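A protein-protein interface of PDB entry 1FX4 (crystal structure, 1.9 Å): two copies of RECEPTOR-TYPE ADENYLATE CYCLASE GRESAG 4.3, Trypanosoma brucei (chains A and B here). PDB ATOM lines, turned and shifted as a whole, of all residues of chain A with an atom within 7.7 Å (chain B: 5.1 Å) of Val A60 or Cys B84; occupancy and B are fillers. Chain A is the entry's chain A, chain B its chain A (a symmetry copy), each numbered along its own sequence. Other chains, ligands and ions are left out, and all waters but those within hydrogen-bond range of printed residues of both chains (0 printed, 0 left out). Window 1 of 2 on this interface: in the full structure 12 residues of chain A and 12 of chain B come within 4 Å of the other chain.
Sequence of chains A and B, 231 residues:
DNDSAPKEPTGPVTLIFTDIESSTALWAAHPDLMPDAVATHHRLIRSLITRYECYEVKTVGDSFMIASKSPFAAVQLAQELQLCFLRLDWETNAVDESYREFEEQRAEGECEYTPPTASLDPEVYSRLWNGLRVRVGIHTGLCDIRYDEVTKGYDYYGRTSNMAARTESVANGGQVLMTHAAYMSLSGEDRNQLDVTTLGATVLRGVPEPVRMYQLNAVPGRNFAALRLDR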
ATOM      1  N   PHE A  17       0.560   5.855  10.101  1.00  0.00           N
ATOM      2  CA  PHE A  17       1.405   4.691   9.890  1.00  0.00           C
ATOM      3  C   PHE A  17       0.634   3.747   8.974  1.00  0.00           C
ATOM      4  O   PHE A  17      -0.571   3.582   9.123  1.00  0.00           O
ATOM      5  CB  PHE A  17       1.751   3.973  11.207  1.00  0.00           C
ATOM      6  CG  PHE A  17       2.936   4.561  11.922  1.00  0.00           C
ATOM      7  CD1 PHE A  17       2.771   5.616  12.800  1.00  0.00           C
ATOM      8  CD2 PHE A  17       4.215   4.050  11.719  1.00  0.00           C
ATOM      9  CE1 PHE A  17       3.866   6.153  13.476  1.00  0.00           C
ATOM     10  CE2 PHE A  17       5.315   4.588  12.396  1.00  0.00           C
ATOM     11  CZ  PHE A  17       5.131   5.637  13.274  1.00  0.00           C
ATOM     12  N   THR A  18       1.326   3.157   8.007  1.00  0.00           N
ATOM     13  CA  THR A  18       0.691   2.213   7.099  1.00  0.00           C
ATOM     14  C   THR A  18       1.521   0.962   6.997  1.00  0.00           C
ATOM     15  O   THR A  18       2.717   0.991   7.265  1.00  0.00           O
ATOM     16  CB  THR A  18       0.591   2.756   5.663  1.00  0.00           C
ATOM     17  OG1 THR A  18       1.888   2.748   5.042  1.00  0.00           O
ATOM     18  CG2 THR A  18       0.030   4.183   5.653  1.00  0.00           C
ATOM     19  N   ASP A  19       0.882  -0.133   6.616  1.00  0.00           N
ATOM     20  CA  ASP A  19       1.612  -1.353   6.373  1.00  0.00           C
ATOM     21  C   ASP A  19       0.763  -2.219   5.472  1.00  0.00           C
ATOM     22  O   ASP A  19      -0.466  -2.098   5.472  1.00  0.00           O
ATOM     23  CB  ASP A  19       1.955  -2.086   7.664  1.00  0.00           C
ATOM     24  CG  ASP A  19       3.232  -2.906   7.532  1.00  0.00           C
ATOM     25  OD1 ASP A  19       3.718  -3.081   6.400  1.00  0.00           O
ATOM     26  OD2 ASP A  19       3.767  -3.357   8.560  1.00  0.00           O
ATOM     27  N   HIS A  42       4.254   1.978  -3.348  1.00  0.00           N
ATOM     28  CA  HIS A  42       5.067   3.145  -2.961  1.00  0.00           C
ATOM     29  C   HIS A  42       4.770   4.372  -3.823  1.00  0.00           C
ATOM     30  O   HIS A  42       4.716   5.497  -3.326  1.00  0.00           O
ATOM     31  CB  HIS A  42       6.556   2.840  -3.036  1.00  0.00           C
ATOM     32  CG  HIS A  42       7.067   2.059  -1.865  1.00  0.00           C
ATOM     33  ND1 HIS A  42       6.291   1.144  -1.191  1.00  0.00           N
ATOM     34  CD2 HIS A  42       8.262   2.080  -1.229  1.00  0.00           C
ATOM     35  CE1 HIS A  42       6.983   0.633  -0.188  1.00  0.00           C
ATOM     36  NE2 HIS A  42       8.185   1.184  -0.188  1.00  0.00           N
ATOM     37  N   GLU A  56       6.815  12.524   4.175  1.00  0.00           N
ATOM     38  CA  GLU A  56       7.250  11.138   4.337  1.00  0.00           C
ATOM     39  C   GLU A  56       8.418  11.141   5.321  1.00  0.00           C
ATOM     40  O   GLU A  56       9.511  11.654   5.011  1.00  0.00           O
ATOM     41  CB  GLU A  56       7.703  10.548   2.996  1.00  0.00           C
ATOM     42  CG  GLU A  56       8.297   9.166   3.121  1.00  0.00           C
ATOM     43  CD  GLU A  56       8.723   8.572   1.783  1.00  0.00           C
ATOM     44  OE1 GLU A  56       9.564   7.645   1.783  1.00  0.00           O
ATOM     45  OE2 GLU A  56       8.212   9.013   0.733  1.00  0.00           O
ATOM     46  N   LYS A  58       9.673   8.259   6.959  1.00  0.00           N
ATOM     47  CA  LYS A  58      10.509   7.120   6.635  1.00  0.00           C
ATOM     48  C   LYS A  58       9.684   5.971   6.093  1.00  0.00           C
ATOM     49  O   LYS A  58       8.463   5.920   6.229  1.00  0.00           O
ATOM     50  CB  LYS A  58      11.244   6.635   7.885  1.00  0.00           C
ATOM     51  CG  LYS A  58      10.325   5.983   8.901  1.00  0.00           C
ATOM     52  CD  LYS A  58      11.034   5.711  10.215  1.00  0.00           C
ATOM     53  CE  LYS A  58      11.351   6.998  10.935  1.00  0.00           C
ATOM     54  NZ  LYS A  58      12.060   6.723  12.211  1.00  0.00           N
ATOM     55  N   THR A  59      10.402   5.008   5.548  1.00  0.00           N
ATOM     56  CA  THR A  59       9.840   3.801   4.985  1.00  0.00           C
ATOM     57  C   THR A  59      10.578   2.647   5.696  1.00  0.00           C
ATOM     58  O   THR A  59      11.790   2.708   5.878  1.00  0.00           O
ATOM     59  CB  THR A  59      10.133   3.780   3.464  1.00  0.00           C
ATOM     60  OG1 THR A  59       9.053   4.411   2.753  1.00  0.00           O
ATOM     61  CG2 THR A  59      10.341   2.396   2.968  1.00  0.00           C
ATOM     62  N   VAL A  60       9.835   1.663   6.191  1.00  0.00           N
ATOM     63  CA  VAL A  60      10.457   0.505   6.852  1.00  0.00           C
ATOM     64  C   VAL A  60       9.775  -0.688   6.204  1.00  0.00           C
ATOM     65  O   VAL A  60       8.627  -0.996   6.517  1.00  0.00           O
ATOM     66  CB  VAL A  60      10.199   0.483   8.369  1.00  0.00           C
ATOM     67  CG1 VAL A  60      10.923  -0.706   9.012  1.00  0.00           C
ATOM     68  CG2 VAL A  60      10.687   1.783   9.016  1.00  0.00           C
ATOM     69  N   GLY A  61      10.476  -1.328   5.274  1.00  0.00           N
ATOM     70  CA  GLY A  61       9.892  -2.446   4.552  1.00  0.00           C
ATOM     71  C   GLY A  61       8.812  -1.803   3.707  1.00  0.00           C
ATOM     72  O   GLY A  61       9.068  -0.777   3.066  1.00  0.00           O
ATOM     73  N   ASP A  62       7.594  -2.327   3.751  1.00  0.00           N
ATOM     74  CA  ASP A  62       6.527  -1.708   2.978  1.00  0.00           C
ATOM     75  C   ASP A  62       5.668  -0.813   3.848  1.00  0.00           C
ATOM     76  O   ASP A  62       4.534  -0.483   3.498  1.00  0.00           O
ATOM     77  CB  ASP A  62       5.686  -2.756   2.261  1.00  0.00           C
ATOM     78  CG  ASP A  62       5.523  -4.019   3.059  1.00  0.00           C
ATOM     79  OD1 ASP A  62       5.337  -3.938   4.290  1.00  0.00           O
ATOM     80  OD2 ASP A  62       5.582  -5.101   2.446  1.00  0.00           O
ATOM     81  N   SER A  63       6.210  -0.438   5.000  1.00  0.00           N
ATOM     82  CA  SER A  63       5.509   0.424   5.933  1.00  0.00           C
ATOM     83  C   SER A  63       5.889   1.887   5.728  1.00  0.00           C
ATOM     84  O   SER A  63       7.061   2.202   5.497  1.00  0.00           O
ATOM     85  CB  SER A  63       5.839   0.020   7.366  1.00  0.00           C
ATOM     86  OG  SER A  63       5.302   0.950   8.282  1.00  0.00           O
ATOM     87  N   PHE A  64       4.902   2.775   5.790  1.00  0.00           N
ATOM     88  CA  PHE A  64       5.165   4.208   5.651  1.00  0.00           C
ATOM     89  C   PHE A  64       4.858   4.905   6.964  1.00  0.00           C
ATOM     90  O   PHE A  64       3.946   4.512   7.699  1.00  0.00           O
ATOM     91  CB  PHE A  64       4.266   4.855   4.578  1.00  0.00           C
ATOM     92  CG  PHE A  64       4.863   4.868   3.208  1.00  0.00           C
ATOM     93  CD1 PHE A  64       4.702   3.777   2.362  1.00  0.00           C
ATOM     94  CD2 PHE A  64       5.568   5.979   2.754  1.00  0.00           C
ATOM     95  CE1 PHE A  64       5.237   3.789   1.069  1.00  0.00           C
ATOM     96  CE2 PHE A  64       6.108   6.002   1.459  1.00  0.00           C
ATOM     97  CZ  PHE A  64       5.942   4.908   0.620  1.00  0.00           C
ATOM     98  N   MET A  65       5.654   5.919   7.270  1.00  0.00           N
ATOM     99  CA  MET A  65       5.402   6.756   8.427  1.00  0.00           C
ATOM    100  C   MET A  65       5.270   8.133   7.785  1.00  0.00           C
ATOM    101  O   MET A  65       6.197   8.612   7.111  1.00  0.00           O
ATOM    102  CB  MET A  65       6.568   6.758   9.396  1.00  0.00           C
ATOM    103  CG  MET A  65       6.290   7.633  10.610  1.00  0.00           C
ATOM    104  SD  MET A  65       7.671   7.650  11.749  1.00  0.00           S
ATOM    105  CE  MET A  65       7.128   8.944  12.895  1.00  0.00           C
ATOM    106  N   LEU B  44      15.340  -5.959   3.012  1.00  0.00           N
ATOM    107  CA  LEU B  44      15.671  -4.731   3.731  1.00  0.00           C
ATOM    108  C   LEU B  44      17.098  -4.320   3.438  1.00  0.00           C
ATOM    109  O   LEU B  44      17.368  -3.159   3.106  1.00  0.00           O
ATOM    110  CB  LEU B  44      15.506  -4.893   5.244  1.00  0.00           C
ATOM    111  CG  LEU B  44      14.112  -5.204   5.786  1.00  0.00           C
ATOM    112  CD1 LEU B  44      14.205  -5.374   7.298  1.00  0.00           C
ATOM    113  CD2 LEU B  44      13.151  -4.061   5.431  1.00  0.00           C
ATOM    114  N   LEU B  48      18.742  -0.957   1.296  1.00  0.00           N
ATOM    115  CA  LEU B  48      19.735  -0.066   1.891  1.00  0.00           C
ATOM    116  C   LEU B  48      20.967   0.030   1.002  1.00  0.00           C
ATOM    117  O   LEU B  48      21.544   1.119   0.845  1.00  0.00           O
ATOM    118  CB  LEU B  48      20.124  -0.559   3.286  1.00  0.00           C
ATOM    119  CG  LEU B  48      19.001  -0.402   4.310  1.00  0.00           C
ATOM    120  CD1 LEU B  48      19.333  -1.145   5.590  1.00  0.00           C
ATOM    121  CD2 LEU B  48      18.790   1.078   4.587  1.00  0.00           C
ATOM    122  N   GLU B  80      21.272   2.622   9.515  1.00  0.00           N
ATOM    123  CA  GLU B  80      19.902   2.478   9.056  1.00  0.00           C
ATOM    124  C   GLU B  80      19.483   1.014   9.094  1.00  0.00           C
ATOM    125  O   GLU B  80      18.318   0.701   9.321  1.00  0.00           O
ATOM    126  CB  GLU B  80      19.728   3.054   7.652  1.00  0.00           C
ATOM    127  CG  GLU B  80      18.302   3.485   7.370  1.00  0.00           C
ATOM    128  CD  GLU B  80      17.769   4.477   8.412  1.00  0.00           C
ATOM    129  OE1 GLU B  80      16.563   4.387   8.741  1.00  0.00           O
ATOM    130  OE2 GLU B  80      18.553   5.331   8.904  1.00  0.00           O
ATOM    131  N   LEU B  81      20.444   0.117   8.898  1.00  0.00           N
ATOM    132  CA  LEU B  81      20.132  -1.304   8.960  1.00  0.00           C
ATOM    133  C   LEU B  81      19.568  -1.615  10.350  1.00  0.00           C
ATOM    134  O   LEU B  81      18.483  -2.159  10.461  1.00  0.00           O
ATOM    135  CB  LEU B  81      21.381  -2.142   8.664  1.00  0.00           C
ATOM    136  CG  LEU B  81      21.197  -3.664   8.535  1.00  0.00           C
ATOM    137  CD1 LEU B  81      22.424  -4.243   7.845  1.00  0.00           C
ATOM    138  CD2 LEU B  81      20.995  -4.331   9.883  1.00  0.00           C
ATOM    139  N   GLN B  82      20.294  -1.259  11.409  1.00  0.00           N
ATOM    140  CA  GLN B  82      19.824  -1.544  12.764  1.00  0.00           C
ATOM    141  C   GLN B  82      18.451  -0.920  13.059  1.00  0.00           C
ATOM    142  O   GLN B  82      17.561  -1.587  13.634  1.00  0.00           O
ATOM    143  CB  GLN B  82      20.844  -1.081  13.793  1.00  0.00           C
ATOM    144  CG  GLN B  82      22.201  -1.775  13.652  1.00  0.00           C
ATOM    145  CD  GLN B  82      22.100  -3.263  13.911  1.00  0.00           C
ATOM    146  OE1 GLN B  82      21.127  -3.730  14.502  1.00  0.00           O
ATOM    147  NE2 GLN B  82      23.111  -4.016  13.474  1.00  0.00           N
ATOM    148  N   LEU B  83      18.270   0.330  12.625  1.00  0.00           N
ATOM    149  CA  LEU B  83      17.007   1.020  12.843  1.00  0.00           C
ATOM    150  C   LEU B  83      15.843   0.406  12.063  1.00  0.00           C
ATOM    151  O   LEU B  83      14.748   0.255  12.600  1.00  0.00           O
ATOM    152  CB  LEU B  83      17.160   2.506  12.512  1.00  0.00           C
ATOM    153  CG  LEU B  83      18.051   3.259  13.505  1.00  0.00           C
ATOM    154  CD1 LEU B  83      18.471   4.600  12.944  1.00  0.00           C
ATOM    155  CD2 LEU B  83      17.314   3.420  14.850  1.00  0.00           C
ATOM    156  N   CYS B  84      16.084   0.045  10.804  1.00  0.00           N
ATOM    157  CA  CYS B  84      15.054  -0.550   9.962  1.00  0.00           C
ATOM    158  C   CYS B  84      14.600  -1.883  10.540  1.00  0.00           C
ATOM    159  O   CYS B  84      13.412  -2.139  10.675  1.00  0.00           O
ATOM    160  CB  CYS B  84      15.572  -0.754   8.530  1.00  0.00           C
ATOM    161  SG  CYS B  84      15.702   0.819   7.564  1.00  0.00           S
ATOM    162  N   PHE B  85      15.558  -2.720  10.913  1.00  0.00           N
ATOM    163  CA  PHE B  85      15.232  -4.027  11.493  1.00  0.00           C
ATOM    164  C   PHE B  85      14.478  -3.876  12.814  1.00  0.00           C
ATOM    165  O   PHE B  85      13.574  -4.657  13.118  1.00  0.00           O
ATOM    166  CB  PHE B  85      16.515  -4.837  11.701  1.00  0.00           C
ATOM    167  CG  PHE B  85      16.956  -5.590  10.479  1.00  0.00           C
ATOM    168  CD1 PHE B  85      17.366  -4.922   9.331  1.00  0.00           C
ATOM    169  CD2 PHE B  85      16.968  -6.980  10.479  1.00  0.00           C
ATOM    170  CE1 PHE B  85      17.768  -5.628   8.193  1.00  0.00           C
ATOM    171  CE2 PHE B  85      17.368  -7.693   9.340  1.00  0.00           C
ATOM    172  CZ  PHE B  85      17.774  -7.014   8.204  1.00  0.00           C
ATOM    173  N   LEU B  86      14.827  -2.856  13.593  1.00  0.00           N
ATOM    174  CA  LEU B  86      14.159  -2.615  14.872  1.00  0.00           C
ATOM    175  C   LEU B  86      12.714  -2.155  14.670  1.00  0.00           C
ATOM    176  O   LEU B  86      11.808  -2.592  15.375  1.00  0.00           O
ATOM    177  CB  LEU B  86      14.902  -1.539  15.683  1.00  0.00           C
ATOM    178  CG  LEU B  86      14.169  -0.955  16.903  1.00  0.00           C
ATOM    179  CD1 LEU B  86      13.882  -2.052  17.937  1.00  0.00           C
ATOM    180  CD2 LEU B  86      14.987   0.153  17.514  1.00  0.00           C
ATOM    181  N   ARG B  87      12.512  -1.287  13.684  1.00  0.00           N
ATOM    182  CA  ARG B  87      11.187  -0.732  13.421  1.00  0.00           C
ATOM    183  C   ARG B  87      10.221  -1.623  12.656  1.00  0.00           C
ATOM    184  O   ARG B  87       9.008  -1.474  12.795  1.00  0.00           O
ATOM    185  CB  ARG B  87      11.322   0.645  12.758  1.00  0.00           C
ATOM    186  CG  ARG B  87      11.984   1.664  13.681  1.00  0.00           C
ATOM    187  CD  ARG B  87      12.318   2.987  12.983  1.00  0.00           C
ATOM    188  NE  ARG B  87      13.002   3.906  13.899  1.00  0.00           N
ATOM    189  CZ  ARG B  87      13.851   4.868  13.528  1.00  0.00           C
ATOM    190  NH1 ARG B  87      14.137   5.063  12.242  1.00  0.00           N
ATOM    191  NH2 ARG B  87      14.437   5.625  14.452  1.00  0.00           N
ATOM    192  N   LEU B  88      10.741  -2.585  11.893  1.00  0.00           N
ATOM    193  CA  LEU B  88       9.882  -3.477  11.126  1.00  0.00           C
ATOM    194  C   LEU B  88       8.987  -4.369  11.983  1.00  0.00           C
ATOM    195  O   LEU B  88       9.406  -4.829  13.042  1.00  0.00           O
ATOM    196  CB  LEU B  88      10.729  -4.382  10.235  1.00  0.00           C
ATOM    197  CG  LEU B  88       9.852  -5.155   9.250  1.00  0.00           C
ATOM    198  CD1 LEU B  88      10.143  -4.680   7.834  1.00  0.00           C
ATOM    199  CD2 LEU B  88      10.075  -6.652   9.381  1.00  0.00           C
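NZ of Lys A58 lies close to NH1 of Arg B87, 2.7 Å away.
The backbone carbonyl oxygen (O) of Glu B80 sits at hydrogen-bond distance from the side-chain sulfur (SG) of Cys B84, at 3.2 Å.
The backbone carbonyl oxygen of Lys A58 sits at hydrogen-bond distance from the backbone NH of Met A65 (3.0 Å).
Val A60 touches Cys B84.
C of Arg B87 touches CG1 of Val A60, 3.8 Å away.
Leu B88 touches Val A60.
Gly A61 touches Leu B44 (CA to CD2, 3.7 Å).
Gly A61 touches Leu B88 (CA to CD1, 3.98 Å).
Asp A19 touches none of the printed residues of chain B.
Of the printed residues of chain B, Lys A58 touches Arg B87 (2.7 Å).
Val A60 touches just these residues of chain B: Cys B84 (3.3 Å), Arg B87 (3.8 Å) and Leu B88 (3.4 Å).
Of the printed residues of chain B, Gly A61 touches Leu B44 and Leu B88.
Phe A64 touches none of the printed residues of chain B.
Printed residues of chain A within 4 Å of Leu B44: Gly A61.
Cys B84 touches just one residue of chain A: Val A60.
Of the printed residues of chain A, Leu B88 touches Val A60 and Gly A61.
The nearest residue of chain B that does not touch Val A60 is Leu B44 (4.8 Å).
The nearest residue of chain A that does not touch Cys B84 is Thr A59 (4.7 Å).
Hydrophobic or aromatic side chains of chain A that line the printed part of chain B: Val A60.
Along chain A the printed residues that touch a printed residue of chain B span positions 58 to 61.
Printed residues of chain B that touch a printed residue of chain A: Leu B44, Cys B84, Arg B87 and Leu B88.
Along chain B the printed residues that touch a printed residue of chain A span positions 44 to 88.
No position is printed for both chains.
Of the 6 pairs that touch across the chains among the printed residues, none has its exchanged pair printed and touching as well.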
